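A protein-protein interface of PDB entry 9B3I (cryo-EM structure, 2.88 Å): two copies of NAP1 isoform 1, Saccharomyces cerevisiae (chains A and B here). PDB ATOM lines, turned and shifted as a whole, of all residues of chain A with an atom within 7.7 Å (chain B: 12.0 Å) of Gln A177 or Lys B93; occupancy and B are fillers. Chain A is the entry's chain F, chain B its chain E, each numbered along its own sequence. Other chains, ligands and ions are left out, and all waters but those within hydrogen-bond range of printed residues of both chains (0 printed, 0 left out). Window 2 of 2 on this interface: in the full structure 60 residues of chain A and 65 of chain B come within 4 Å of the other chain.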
ATOM      1  N   PRO A 148     -26.648 -20.658  21.925  1.00  0.00           N
ATOM      2  CA  PRO A 148     -27.187 -19.578  21.091  1.00  0.00           C
ATOM      3  C   PRO A 148     -28.556 -19.928  20.527  1.00  0.00           C
ATOM      4  O   PRO A 148     -28.830 -21.074  20.167  1.00  0.00           O
ATOM      5  CB  PRO A 148     -26.142 -19.433  19.978  1.00  0.00           C
ATOM      6  CG  PRO A 148     -24.896 -19.977  20.570  1.00  0.00           C
ATOM      7  CD  PRO A 148     -25.319 -21.096  21.469  1.00  0.00           C
ATOM      8  N   ILE A 153     -28.191 -16.227  16.472  1.00  0.00           N
ATOM      9  CA  ILE A 153     -27.330 -16.811  15.451  1.00  0.00           C
ATOM     10  C   ILE A 153     -27.432 -16.010  14.159  1.00  0.00           C
ATOM     11  O   ILE A 153     -26.421 -15.674  13.534  1.00  0.00           O
ATOM     12  CB  ILE A 153     -27.692 -18.290  15.232  1.00  0.00           C
ATOM     13  CG1 ILE A 153     -27.222 -19.129  16.421  1.00  0.00           C
ATOM     14  CG2 ILE A 153     -27.084 -18.807  13.934  1.00  0.00           C
ATOM     15  CD1 ILE A 153     -27.762 -20.544  16.425  1.00  0.00           C
ATOM     16  N   LEU A 168     -16.890 -17.223  10.781  1.00  0.00           N
ATOM     17  CA  LEU A 168     -18.037 -17.691  11.549  1.00  0.00           C
ATOM     18  C   LEU A 168     -19.144 -18.288  10.690  1.00  0.00           C
ATOM     19  O   LEU A 168     -20.048 -18.926  11.238  1.00  0.00           O
ATOM     20  CB  LEU A 168     -18.595 -16.544  12.389  1.00  0.00           C
ATOM     21  CG  LEU A 168     -17.534 -15.983  13.325  1.00  0.00           C
ATOM     22  CD1 LEU A 168     -18.068 -14.838  14.163  1.00  0.00           C
ATOM     23  CD2 LEU A 168     -17.039 -17.111  14.200  1.00  0.00           C
ATOM     24  N   VAL A 170     -21.152 -20.801   9.060  1.00  0.00           N
ATOM     25  CA  VAL A 170     -21.156 -22.243   9.279  1.00  0.00           C
ATOM     26  C   VAL A 170     -21.243 -22.963   7.941  1.00  0.00           C
ATOM     27  O   VAL A 170     -22.096 -22.649   7.100  1.00  0.00           O
ATOM     28  CB  VAL A 170     -22.314 -22.647  10.204  1.00  0.00           C
ATOM     29  CG1 VAL A 170     -22.365 -24.158  10.358  1.00  0.00           C
ATOM     30  CG2 VAL A 170     -22.172 -21.974  11.559  1.00  0.00           C
ATOM     31  N   ASP A 171     -20.364 -23.938   7.742  1.00  0.00           N
ATOM     32  CA  ASP A 171     -20.299 -24.681   6.495  1.00  0.00           C
ATOM     33  C   ASP A 171     -21.187 -25.924   6.555  1.00  0.00           C
ATOM     34  O   ASP A 171     -21.714 -26.302   7.603  1.00  0.00           O
ATOM     35  CB  ASP A 171     -18.855 -25.068   6.182  1.00  0.00           C
ATOM     36  CG  ASP A 171     -17.920 -23.876   6.192  1.00  0.00           C
ATOM     37  OD1 ASP A 171     -18.277 -22.834   5.604  1.00  0.00           O
ATOM     38  OD2 ASP A 171     -16.827 -23.980   6.786  1.00  0.00           O
ATOM     39  N   GLU A 172     -21.348 -26.562   5.392  1.00  0.00           N
ATOM     40  CA  GLU A 172     -22.192 -27.749   5.300  1.00  0.00           C
ATOM     41  C   GLU A 172     -21.624 -28.904   6.115  1.00  0.00           C
ATOM     42  O   GLU A 172     -22.379 -29.694   6.694  1.00  0.00           O
ATOM     43  CB  GLU A 172     -22.357 -28.156   3.834  1.00  0.00           C
ATOM     44  CG  GLU A 172     -23.266 -29.355   3.612  1.00  0.00           C
ATOM     45  CD  GLU A 172     -24.703 -29.086   4.019  1.00  0.00           C
ATOM     46  OE1 GLU A 172     -25.120 -27.907   4.005  1.00  0.00           O
ATOM     47  OE2 GLU A 172     -25.415 -30.057   4.351  1.00  0.00           O
ATOM     48  N   GLU A 173     -20.294 -29.027   6.162  1.00  0.00           N
ATOM     49  CA  GLU A 173     -19.676 -30.148   6.867  1.00  0.00           C
ATOM     50  C   GLU A 173     -20.032 -30.141   8.351  1.00  0.00           C
ATOM     51  O   GLU A 173     -20.227 -31.202   8.953  1.00  0.00           O
ATOM     52  CB  GLU A 173     -18.157 -30.122   6.671  1.00  0.00           C
ATOM     53  CG  GLU A 173     -17.467 -28.867   7.187  1.00  0.00           C
ATOM     54  CD  GLU A 173     -15.957 -28.919   7.043  1.00  0.00           C
ATOM     55  OE1 GLU A 173     -15.298 -29.554   7.893  1.00  0.00           O
ATOM     56  OE2 GLU A 173     -15.426 -28.310   6.089  1.00  0.00           O
ATOM     57  N   GLU A 174     -20.127 -28.955   8.957  1.00  0.00           N
ATOM     58  CA  GLU A 174     -20.423 -28.885  10.384  1.00  0.00           C
ATOM     59  C   GLU A 174     -21.896 -29.164  10.668  1.00  0.00           C
ATOM     60  O   GLU A 174     -22.232 -29.712  11.724  1.00  0.00           O
ATOM     61  CB  GLU A 174     -20.008 -27.524  10.937  1.00  0.00           C
ATOM     62  CG  GLU A 174     -18.572 -27.157  10.620  1.00  0.00           C
ATOM     63  CD  GLU A 174     -18.308 -25.671  10.746  1.00  0.00           C
ATOM     64  OE1 GLU A 174     -18.439 -25.133  11.864  1.00  0.00           O
ATOM     65  OE2 GLU A 174     -17.974 -25.041   9.721  1.00  0.00           O
ATOM     66  N   LYS A 175     -22.790 -28.785   9.749  1.00  0.00           N
ATOM     67  CA  LYS A 175     -24.213 -29.040   9.961  1.00  0.00           C
ATOM     68  C   LYS A 175     -24.518 -30.532  10.031  1.00  0.00           C
ATOM     69  O   LYS A 175     -25.498 -30.935  10.669  1.00  0.00           O
ATOM     70  CB  LYS A 175     -25.046 -28.373   8.864  1.00  0.00           C
ATOM     71  CG  LYS A 175     -24.882 -26.863   8.793  1.00  0.00           C
ATOM     72  CD  LYS A 175     -25.248 -26.317   7.421  1.00  0.00           C
ATOM     73  CE  LYS A 175     -24.795 -24.867   7.273  1.00  0.00           C
ATOM     74  NZ  LYS A 175     -24.297 -24.539   5.905  1.00  0.00           N
ATOM     75  N   ALA A 176     -23.702 -31.364   9.380  1.00  0.00           N
ATOM     76  CA  ALA A 176     -23.864 -32.808   9.498  1.00  0.00           C
ATOM     77  C   ALA A 176     -23.521 -33.319  10.891  1.00  0.00           C
ATOM     78  O   ALA A 176     -23.958 -34.414  11.261  1.00  0.00           O
ATOM     79  CB  ALA A 176     -23.003 -33.520   8.454  1.00  0.00           C
ATOM     80  N   GLN A 177     -22.753 -32.557  11.666  1.00  0.00           N
ATOM     81  CA  GLN A 177     -22.394 -32.968  13.014  1.00  0.00           C
ATOM     82  C   GLN A 177     -23.613 -32.915  13.931  1.00  0.00           C
ATOM     83  O   GLN A 177     -24.628 -32.280  13.631  1.00  0.00           O
ATOM     84  CB  GLN A 177     -21.283 -32.079  13.572  1.00  0.00           C
ATOM     85  CG  GLN A 177     -20.006 -32.061  12.747  1.00  0.00           C
ATOM     86  CD  GLN A 177     -19.086 -30.914  13.123  1.00  0.00           C
ATOM     87  OE1 GLN A 177     -19.542 -29.842  13.519  1.00  0.00           O
ATOM     88  NE2 GLN A 177     -17.782 -31.137  13.005  1.00  0.00           N
ATOM     89  N   ASN A 178     -23.499 -33.596  15.067  1.00  0.00           N
ATOM     90  CA  ASN A 178     -24.567 -33.674  16.051  1.00  0.00           C
ATOM     91  C   ASN A 178     -24.122 -33.023  17.353  1.00  0.00           C
ATOM     92  O   ASN A 178     -22.926 -32.952  17.652  1.00  0.00           O
ATOM     93  CB  ASN A 178     -24.980 -35.127  16.309  1.00  0.00           C
ATOM     94  CG  ASN A 178     -25.423 -35.839  15.048  1.00  0.00           C
ATOM     95  OD1 ASN A 178     -26.608 -35.864  14.718  1.00  0.00           O
ATOM     96  ND2 ASN A 178     -24.470 -36.428  14.335  1.00  0.00           N
ATOM     97  N   ASP A 179     -25.101 -32.540  18.122  1.00  0.00           N
ATOM     98  CA  ASP A 179     -24.794 -31.884  19.389  1.00  0.00           C
ATOM     99  C   ASP A 179     -24.069 -32.818  20.350  1.00  0.00           C
ATOM    100  O   ASP A 179     -23.207 -32.370  21.114  1.00  0.00           O
ATOM    101  CB  ASP A 179     -26.077 -31.347  20.029  1.00  0.00           C
ATOM    102  CG  ASP A 179     -27.099 -32.438  20.313  1.00  0.00           C
ATOM    103  OD1 ASP A 179     -26.848 -33.612  19.963  1.00  0.00           O
ATOM    104  OD2 ASP A 179     -28.158 -32.120  20.892  1.00  0.00           O
ATOM    105  N   SER A 180     -24.397 -34.112  20.323  1.00  0.00           N
ATOM    106  CA  SER A 180     -23.749 -35.059  21.225  1.00  0.00           C
ATOM    107  C   SER A 180     -22.245 -35.108  20.989  1.00  0.00           C
ATOM    108  O   SER A 180     -21.458 -35.134  21.943  1.00  0.00           O
ATOM    109  CB  SER A 180     -24.365 -36.448  21.056  1.00  0.00           C
ATOM    110  OG  SER A 180     -24.246 -36.898  19.718  1.00  0.00           O
ATOM    111  N   GLU A 181     -21.825 -35.124  19.722  1.00  0.00           N
ATOM    112  CA  GLU A 181     -20.399 -35.085  19.418  1.00  0.00           C
ATOM    113  C   GLU A 181     -19.794 -33.732  19.774  1.00  0.00           C
ATOM    114  O   GLU A 181     -18.669 -33.662  20.284  1.00  0.00           O
ATOM    115  CB  GLU A 181     -20.169 -35.401  17.940  1.00  0.00           C
ATOM    116  CG  GLU A 181     -20.767 -36.721  17.481  1.00  0.00           C
ATOM    117  CD  GLU A 181     -20.722 -36.888  15.975  1.00  0.00           C
ATOM    118  OE1 GLU A 181     -19.707 -37.402  15.462  1.00  0.00           O
ATOM    119  OE2 GLU A 181     -21.703 -36.504  15.302  1.00  0.00           O
ATOM    120  N   GLU A 182     -20.525 -32.647  19.511  1.00  0.00           N
ATOM    121  CA  GLU A 182     -19.982 -31.311  19.739  1.00  0.00           C
ATOM    122  C   GLU A 182     -19.925 -30.971  21.225  1.00  0.00           C
ATOM    123  O   GLU A 182     -18.947 -30.378  21.692  1.00  0.00           O
ATOM    124  CB  GLU A 182     -20.811 -30.274  18.984  1.00  0.00           C
ATOM    125  CG  GLU A 182     -20.824 -30.475  17.480  1.00  0.00           C
ATOM    126  CD  GLU A 182     -21.622 -29.408  16.760  1.00  0.00           C
ATOM    127  OE1 GLU A 182     -21.253 -28.219  16.862  1.00  0.00           O
ATOM    128  OE2 GLU A 182     -22.617 -29.759  16.093  1.00  0.00           O
ATOM    129  N   GLY B  86      -8.634 -18.655  13.393  1.00  0.00           N
ATOM    130  CA  GLY B  86      -8.538 -19.640  12.333  1.00  0.00           C
ATOM    131  C   GLY B  86      -9.077 -20.998  12.734  1.00  0.00           C
ATOM    132  O   GLY B  86     -10.162 -21.395  12.308  1.00  0.00           O
ATOM    133  N   TYR B  87      -8.312 -21.716  13.561  1.00  0.00           N
ATOM    134  CA  TYR B  87      -8.761 -23.022  14.035  1.00  0.00           C
ATOM    135  C   TYR B  87     -10.015 -22.910  14.891  1.00  0.00           C
ATOM    136  O   TYR B  87     -10.736 -23.899  15.065  1.00  0.00           O
ATOM    137  CB  TYR B  87      -7.646 -23.721  14.811  1.00  0.00           C
ATOM    138  CG  TYR B  87      -7.929 -25.183  15.066  1.00  0.00           C
ATOM    139  CD1 TYR B  87      -8.132 -26.064  14.011  1.00  0.00           C
ATOM    140  CD2 TYR B  87      -8.007 -25.681  16.359  1.00  0.00           C
ATOM    141  CE1 TYR B  87      -8.399 -27.401  14.238  1.00  0.00           C
ATOM    142  CE2 TYR B  87      -8.271 -27.017  16.595  1.00  0.00           C
ATOM    143  CZ  TYR B  87      -8.467 -27.871  15.532  1.00  0.00           C
ATOM    144  OH  TYR B  87      -8.731 -29.202  15.765  1.00  0.00           O
ATOM    145  N   VAL B  88     -10.282 -21.726  15.448  1.00  0.00           N
ATOM    146  CA  VAL B  88     -11.551 -21.503  16.135  1.00  0.00           C
ATOM    147  C   VAL B  88     -12.709 -21.701  15.168  1.00  0.00           C
ATOM    148  O   VAL B  88     -13.739 -22.291  15.517  1.00  0.00           O
ATOM    149  CB  VAL B  88     -11.576 -20.100  16.772  1.00  0.00           C
ATOM    150  CG1 VAL B  88     -12.790 -19.943  17.666  1.00  0.00           C
ATOM    151  CG2 VAL B  88     -10.302 -19.852  17.560  1.00  0.00           C
ATOM    152  N   GLY B  89     -12.558 -21.217  13.934  1.00  0.00           N
ATOM    153  CA  GLY B  89     -13.532 -21.527  12.903  1.00  0.00           C
ATOM    154  C   GLY B  89     -13.526 -22.996  12.523  1.00  0.00           C
ATOM    155  O   GLY B  89     -14.580 -23.591  12.289  1.00  0.00           O
ATOM    156  N   GLY B  90     -12.339 -23.603  12.458  1.00  0.00           N
ATOM    157  CA  GLY B  90     -12.245 -25.017  12.140  1.00  0.00           C
ATOM    158  C   GLY B  90     -12.892 -25.921  13.168  1.00  0.00           C
ATOM    159  O   GLY B  90     -13.155 -27.092  12.876  1.00  0.00           O
ATOM    160  N   LEU B  91     -13.152 -25.406  14.367  1.00  0.00           N
ATOM    161  CA  LEU B  91     -13.838 -26.170  15.389  1.00  0.00           C
ATOM    162  C   LEU B  91     -15.296 -26.387  14.980  1.00  0.00           C
ATOM    163  O   LEU B  91     -15.817 -25.676  14.117  1.00  0.00           O
ATOM    164  CB  LEU B  91     -13.745 -25.441  16.728  1.00  0.00           C
ATOM    165  CG  LEU B  91     -12.446 -25.614  17.518  1.00  0.00           C
ATOM    166  CD1 LEU B  91     -12.476 -24.777  18.790  1.00  0.00           C
ATOM    167  CD2 LEU B  91     -12.205 -27.080  17.840  1.00  0.00           C
ATOM    168  N   PRO B  92     -15.978 -27.394  15.575  1.00  0.00           N
ATOM    169  CA  PRO B  92     -17.363 -27.695  15.170  1.00  0.00           C
ATOM    170  C   PRO B  92     -18.311 -26.507  15.267  1.00  0.00           C
ATOM    171  O   PRO B  92     -17.982 -25.488  15.882  1.00  0.00           O
ATOM    172  CB  PRO B  92     -17.774 -28.817  16.135  1.00  0.00           C
ATOM    173  CG  PRO B  92     -16.491 -29.439  16.564  1.00  0.00           C
ATOM    174  CD  PRO B  92     -15.489 -28.331  16.602  1.00  0.00           C
ATOM    175  N   LYS B  93     -19.502 -26.639  14.671  1.00  0.00           N
ATOM    176  CA  LYS B  93     -20.411 -25.507  14.517  1.00  0.00           C
ATOM    177  C   LYS B  93     -20.930 -24.965  15.841  1.00  0.00           C
ATOM    178  O   LYS B  93     -21.498 -23.868  15.853  1.00  0.00           O
ATOM    179  CB  LYS B  93     -21.596 -25.881  13.625  1.00  0.00           C
ATOM    180  CG  LYS B  93     -22.264 -27.200  13.959  1.00  0.00           C
ATOM    181  CD  LYS B  93     -23.600 -27.321  13.239  1.00  0.00           C
ATOM    182  CE  LYS B  93     -24.471 -28.395  13.862  1.00  0.00           C
ATOM    183  NZ  LYS B  93     -23.792 -29.720  13.835  1.00  0.00           N
ATOM    184  N   ASN B  94     -20.761 -25.694  16.944  1.00  0.00           N
ATOM    185  CA  ASN B  94     -21.053 -25.117  18.251  1.00  0.00           C
ATOM    186  C   ASN B  94     -20.197 -23.877  18.481  1.00  0.00           C
ATOM    187  O   ASN B  94     -20.675 -22.859  18.994  1.00  0.00           O
ATOM    188  CB  ASN B  94     -20.816 -26.156  19.350  1.00  0.00           C
ATOM    189  CG  ASN B  94     -21.284 -25.686  20.719  1.00  0.00           C
ATOM    190  OD1 ASN B  94     -21.765 -24.564  20.879  1.00  0.00           O
ATOM    191  ND2 ASN B  94     -21.143 -26.551  21.717  1.00  0.00           N
ATOM    192  N   VAL B  95     -18.923 -23.947  18.094  1.00  0.00           N
ATOM    193  CA  VAL B  95     -18.033 -22.806  18.266  1.00  0.00           C
ATOM    194  C   VAL B  95     -18.476 -21.631  17.402  1.00  0.00           C
ATOM    195  O   VAL B  95     -18.518 -20.484  17.867  1.00  0.00           O
ATOM    196  CB  VAL B  95     -16.581 -23.226  17.977  1.00  0.00           C
ATOM    197  CG1 VAL B  95     -15.641 -22.045  18.135  1.00  0.00           C
ATOM    198  CG2 VAL B  95     -16.184 -24.344  18.926  1.00  0.00           C
ATOM    199  N   LYS B  96     -18.825 -21.888  16.140  1.00  0.00           N
ATOM    200  CA  LYS B  96     -19.294 -20.790  15.302  1.00  0.00           C
ATOM    201  C   LYS B  96     -20.581 -20.182  15.839  1.00  0.00           C
ATOM    202  O   LYS B  96     -20.721 -18.959  15.854  1.00  0.00           O
ATOM    203  CB  LYS B  96     -19.472 -21.229  13.849  1.00  0.00           C
ATOM    204  CG  LYS B  96     -18.177 -21.551  13.130  1.00  0.00           C
ATOM    205  CD  LYS B  96     -18.447 -21.939  11.689  1.00  0.00           C
ATOM    206  CE  LYS B  96     -17.163 -22.281  10.956  1.00  0.00           C
ATOM    207  NZ  LYS B  96     -17.409 -22.677   9.541  1.00  0.00           N
ATOM    208  N   GLU B  97     -21.534 -21.005  16.285  1.00  0.00           N
ATOM    209  CA  GLU B  97     -22.789 -20.432  16.763  1.00  0.00           C
ATOM    210  C   GLU B  97     -22.584 -19.641  18.052  1.00  0.00           C
ATOM    211  O   GLU B  97     -23.165 -18.561  18.219  1.00  0.00           O
ATOM    212  CB  GLU B  97     -23.851 -21.520  16.947  1.00  0.00           C
ATOM    213  CG  GLU B  97     -23.558 -22.540  18.025  1.00  0.00           C
ATOM    214  CD  GLU B  97     -24.615 -23.618  18.111  1.00  0.00           C
ATOM    215  OE1 GLU B  97     -25.572 -23.582  17.310  1.00  0.00           O
ATOM    216  OE2 GLU B  97     -24.486 -24.503  18.982  1.00  0.00           O
ATOM    217  N   LYS B  98     -21.744 -20.142  18.966  1.00  0.00           N
ATOM    218  CA  LYS B  98     -21.471 -19.385  20.182  1.00  0.00           C
ATOM    219  C   LYS B  98     -20.783 -18.064  19.867  1.00  0.00           C
ATOM    220  O   LYS B  98     -21.108 -17.032  20.462  1.00  0.00           O
ATOM    221  CB  LYS B  98     -20.653 -20.216  21.178  1.00  0.00           C
ATOM    222  CG  LYS B  98     -19.230 -20.544  20.769  1.00  0.00           C
ATOM    223  CD  LYS B  98     -18.508 -21.381  21.818  1.00  0.00           C
ATOM    224  CE  LYS B  98     -17.106 -21.731  21.345  1.00  0.00           C
ATOM    225  NZ  LYS B  98     -16.204 -20.553  21.221  1.00  0.00           N
ATOM    226  N   LEU B  99     -19.839 -18.061  18.924  1.00  0.00           N
ATOM    227  CA  LEU B  99     -19.150 -16.805  18.654  1.00  0.00           C
ATOM    228  C   LEU B  99     -20.015 -15.862  17.812  1.00  0.00           C
ATOM    229  O   LEU B  99     -19.858 -14.641  17.899  1.00  0.00           O
ATOM    230  CB  LEU B  99     -17.783 -17.082  18.023  1.00  0.00           C
ATOM    231  CG  LEU B  99     -16.909 -15.860  17.759  1.00  0.00           C
ATOM    232  CD1 LEU B  99     -16.617 -15.214  19.087  1.00  0.00           C
ATOM    233  CD2 LEU B  99     -15.592 -16.282  17.149  1.00  0.00           C
ATOM    234  N   LEU B 100     -20.948 -16.399  17.018  1.00  0.00           N
ATOM    235  CA  LEU B 100     -21.980 -15.559  16.407  1.00  0.00           C
ATOM    236  C   LEU B 100     -22.835 -14.889  17.468  1.00  0.00           C
ATOM    237  O   LEU B 100     -23.174 -13.703  17.352  1.00  0.00           O
ATOM    238  CB  LEU B 100     -22.878 -16.386  15.485  1.00  0.00           C
ATOM    239  CG  LEU B 100     -22.375 -17.030  14.199  1.00  0.00           C
ATOM    240  CD1 LEU B 100     -23.477 -17.886  13.615  1.00  0.00           C
ATOM    241  CD2 LEU B 100     -21.974 -15.963  13.210  1.00  0.00           C
ATOM    242  N   SER B 101     -23.221 -15.643  18.495  1.00  0.00           N
ATOM    243  CA  SER B 101     -23.933 -15.047  19.617  1.00  0.00           C
ATOM    244  C   SER B 101     -23.081 -13.975  20.285  1.00  0.00           C
ATOM    245  O   SER B 101     -23.593 -12.927  20.697  1.00  0.00           O
ATOM    246  CB  SER B 101     -24.329 -16.132  20.617  1.00  0.00           C
ATOM    247  OG  SER B 101     -23.214 -16.546  21.387  1.00  0.00           O
ATOM    248  N   LEU B 102     -21.774 -14.220  20.394  1.00  0.00           N
ATOM    249  CA  LEU B 102     -20.879 -13.216  20.960  1.00  0.00           C
ATOM    250  C   LEU B 102     -20.853 -11.953  20.106  1.00  0.00           C
ATOM    251  O   LEU B 102     -20.825 -10.841  20.637  1.00  0.00           O
ATOM    252  CB  LEU B 102     -19.468 -13.788  21.120  1.00  0.00           C
ATOM    253  CG  LEU B 102     -19.294 -14.928  22.127  1.00  0.00           C
ATOM    254  CD1 LEU B 102     -17.831 -15.105  22.505  1.00  0.00           C
ATOM    255  CD2 LEU B 102     -20.137 -14.677  23.365  1.00  0.00           C
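The side-chain amide oxygen (OD1) of Asn B94 lies close to the side-chain carboxylate (OE2) of Glu B97, 3.3 Å away.
The backbone carbonyl oxygen (O) of Val A170 sits at hydrogen-bond distance from the side-chain amino group (NZ) of Lys A175 (3.1 Å).
N of Asp A171 sits at hydrogen-bond distance from OE2 of Glu A174, at 3.3 Å.
The side-chain carboxylate (OE1) of Glu A172 is in salt-bridge range of the side-chain amino group (NZ) of Lys A175 (3.95 Å).
O of Glu A174 sits close to OE1 of Gln A177 (3.2 Å).
No position is printed for both chains.
Among the printed residues, pairs that only touch across the chains: Pro A148 with Glu B97, Gln A177 with Pro B92, Leu A168 with Leu B99, Leu A168 with Lys B96, Pro A148 with Lys B98, Leu A168 with Leu B100, Glu A182 with Pro B92, Val A170 with Lys B96, Glu A174 with Pro B92, Ile A153 with Leu B100, Lys A175 with Lys B93, Val A170 with Lys B93, Pro A148 with Ser B101 and Ile A153 with Glu B97.
Of chain B, only Lys B93 and Lys B96 come within 4 Å of Val A170.
Of the printed residues of chain B, Asp A171 touches Lys B96 (3.1 Å).
Of chain B, only Lys B93 comes within 4 Å of Lys A175.
No residue of chain B comes within 4 Å of Ala A176.
Gln A177 touches just these residues of chain B: Pro B92 (3.3 Å) and Lys B93 (2.7 Å).
No residue of chain B comes within 4 Å of Asn A178.
No residue of chain B comes within 4 Å of Glu A181.
Of the printed residues of chain A, Lys B93 touches Val A170 (3.8 Å), Glu A174 (2.6 Å), Lys A175 (3.8 Å), Gln A177 (2.7 Å) and Glu A182 (2.5 Å).
Of the printed residues of chain A, Lys B96 touches Leu A168, Val A170, Asp A171 and Glu A174.
Of the printed residues of chain A, Ser B101 touches Pro A148 (3.8 Å).
The nearest residue of chain B that does not touch Gln A177 is Asn B94 (5.5 Å).
The nearest residue of chain A that does not touch Lys B93 is Asn A178 (4.1 Å).
The nearest printed residue of chain A that does not touch Leu B100 is Val A170 (4.8 Å).
Of the 17 printed residues of chain B, 10 touch a printed residue of chain A.
Of the 16 printed residues of chain A, 9 touch a printed residue of chain B.
Printed residues of chain A that touch a printed residue of chain B: Pro A148, Ile A153, Leu A168, Val A170, Asp A171, Glu A174, Lys A175, Gln A177 and Glu A182.
Hydrophobic or aromatic side chains of chain A that line the printed part of chain B: Pro A148, Ile A153, Leu A168 and Val A170.
O of Glu A174 is in hydrogen-bond range of NZ of Lys B93 (2.6 Å).
O of Gln A177 lies within hydrogen-bond range of NZ of Lys B93 (2.7 Å).
The side-chain amino group (NZ) of Lys B93 is in salt-bridge range of the side-chain carboxylate (OE2) of Glu A182.
The backbone NH (N) of Asn B94 lies within hydrogen-bond range of the side-chain carboxylate (OE1) of Glu A182 (2.6 Å).
The side-chain amino group (NZ) of Lys B96 is in salt-bridge range of the side-chain carboxylate (OD2) of Asp A171.
NZ of Lys B96 is in salt-bridge range of OE2 of Glu A174.
The backbone carbonyl oxygen (O) of Leu B91 sits close to the side-chain carboxylate (OE1) of Glu A174.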
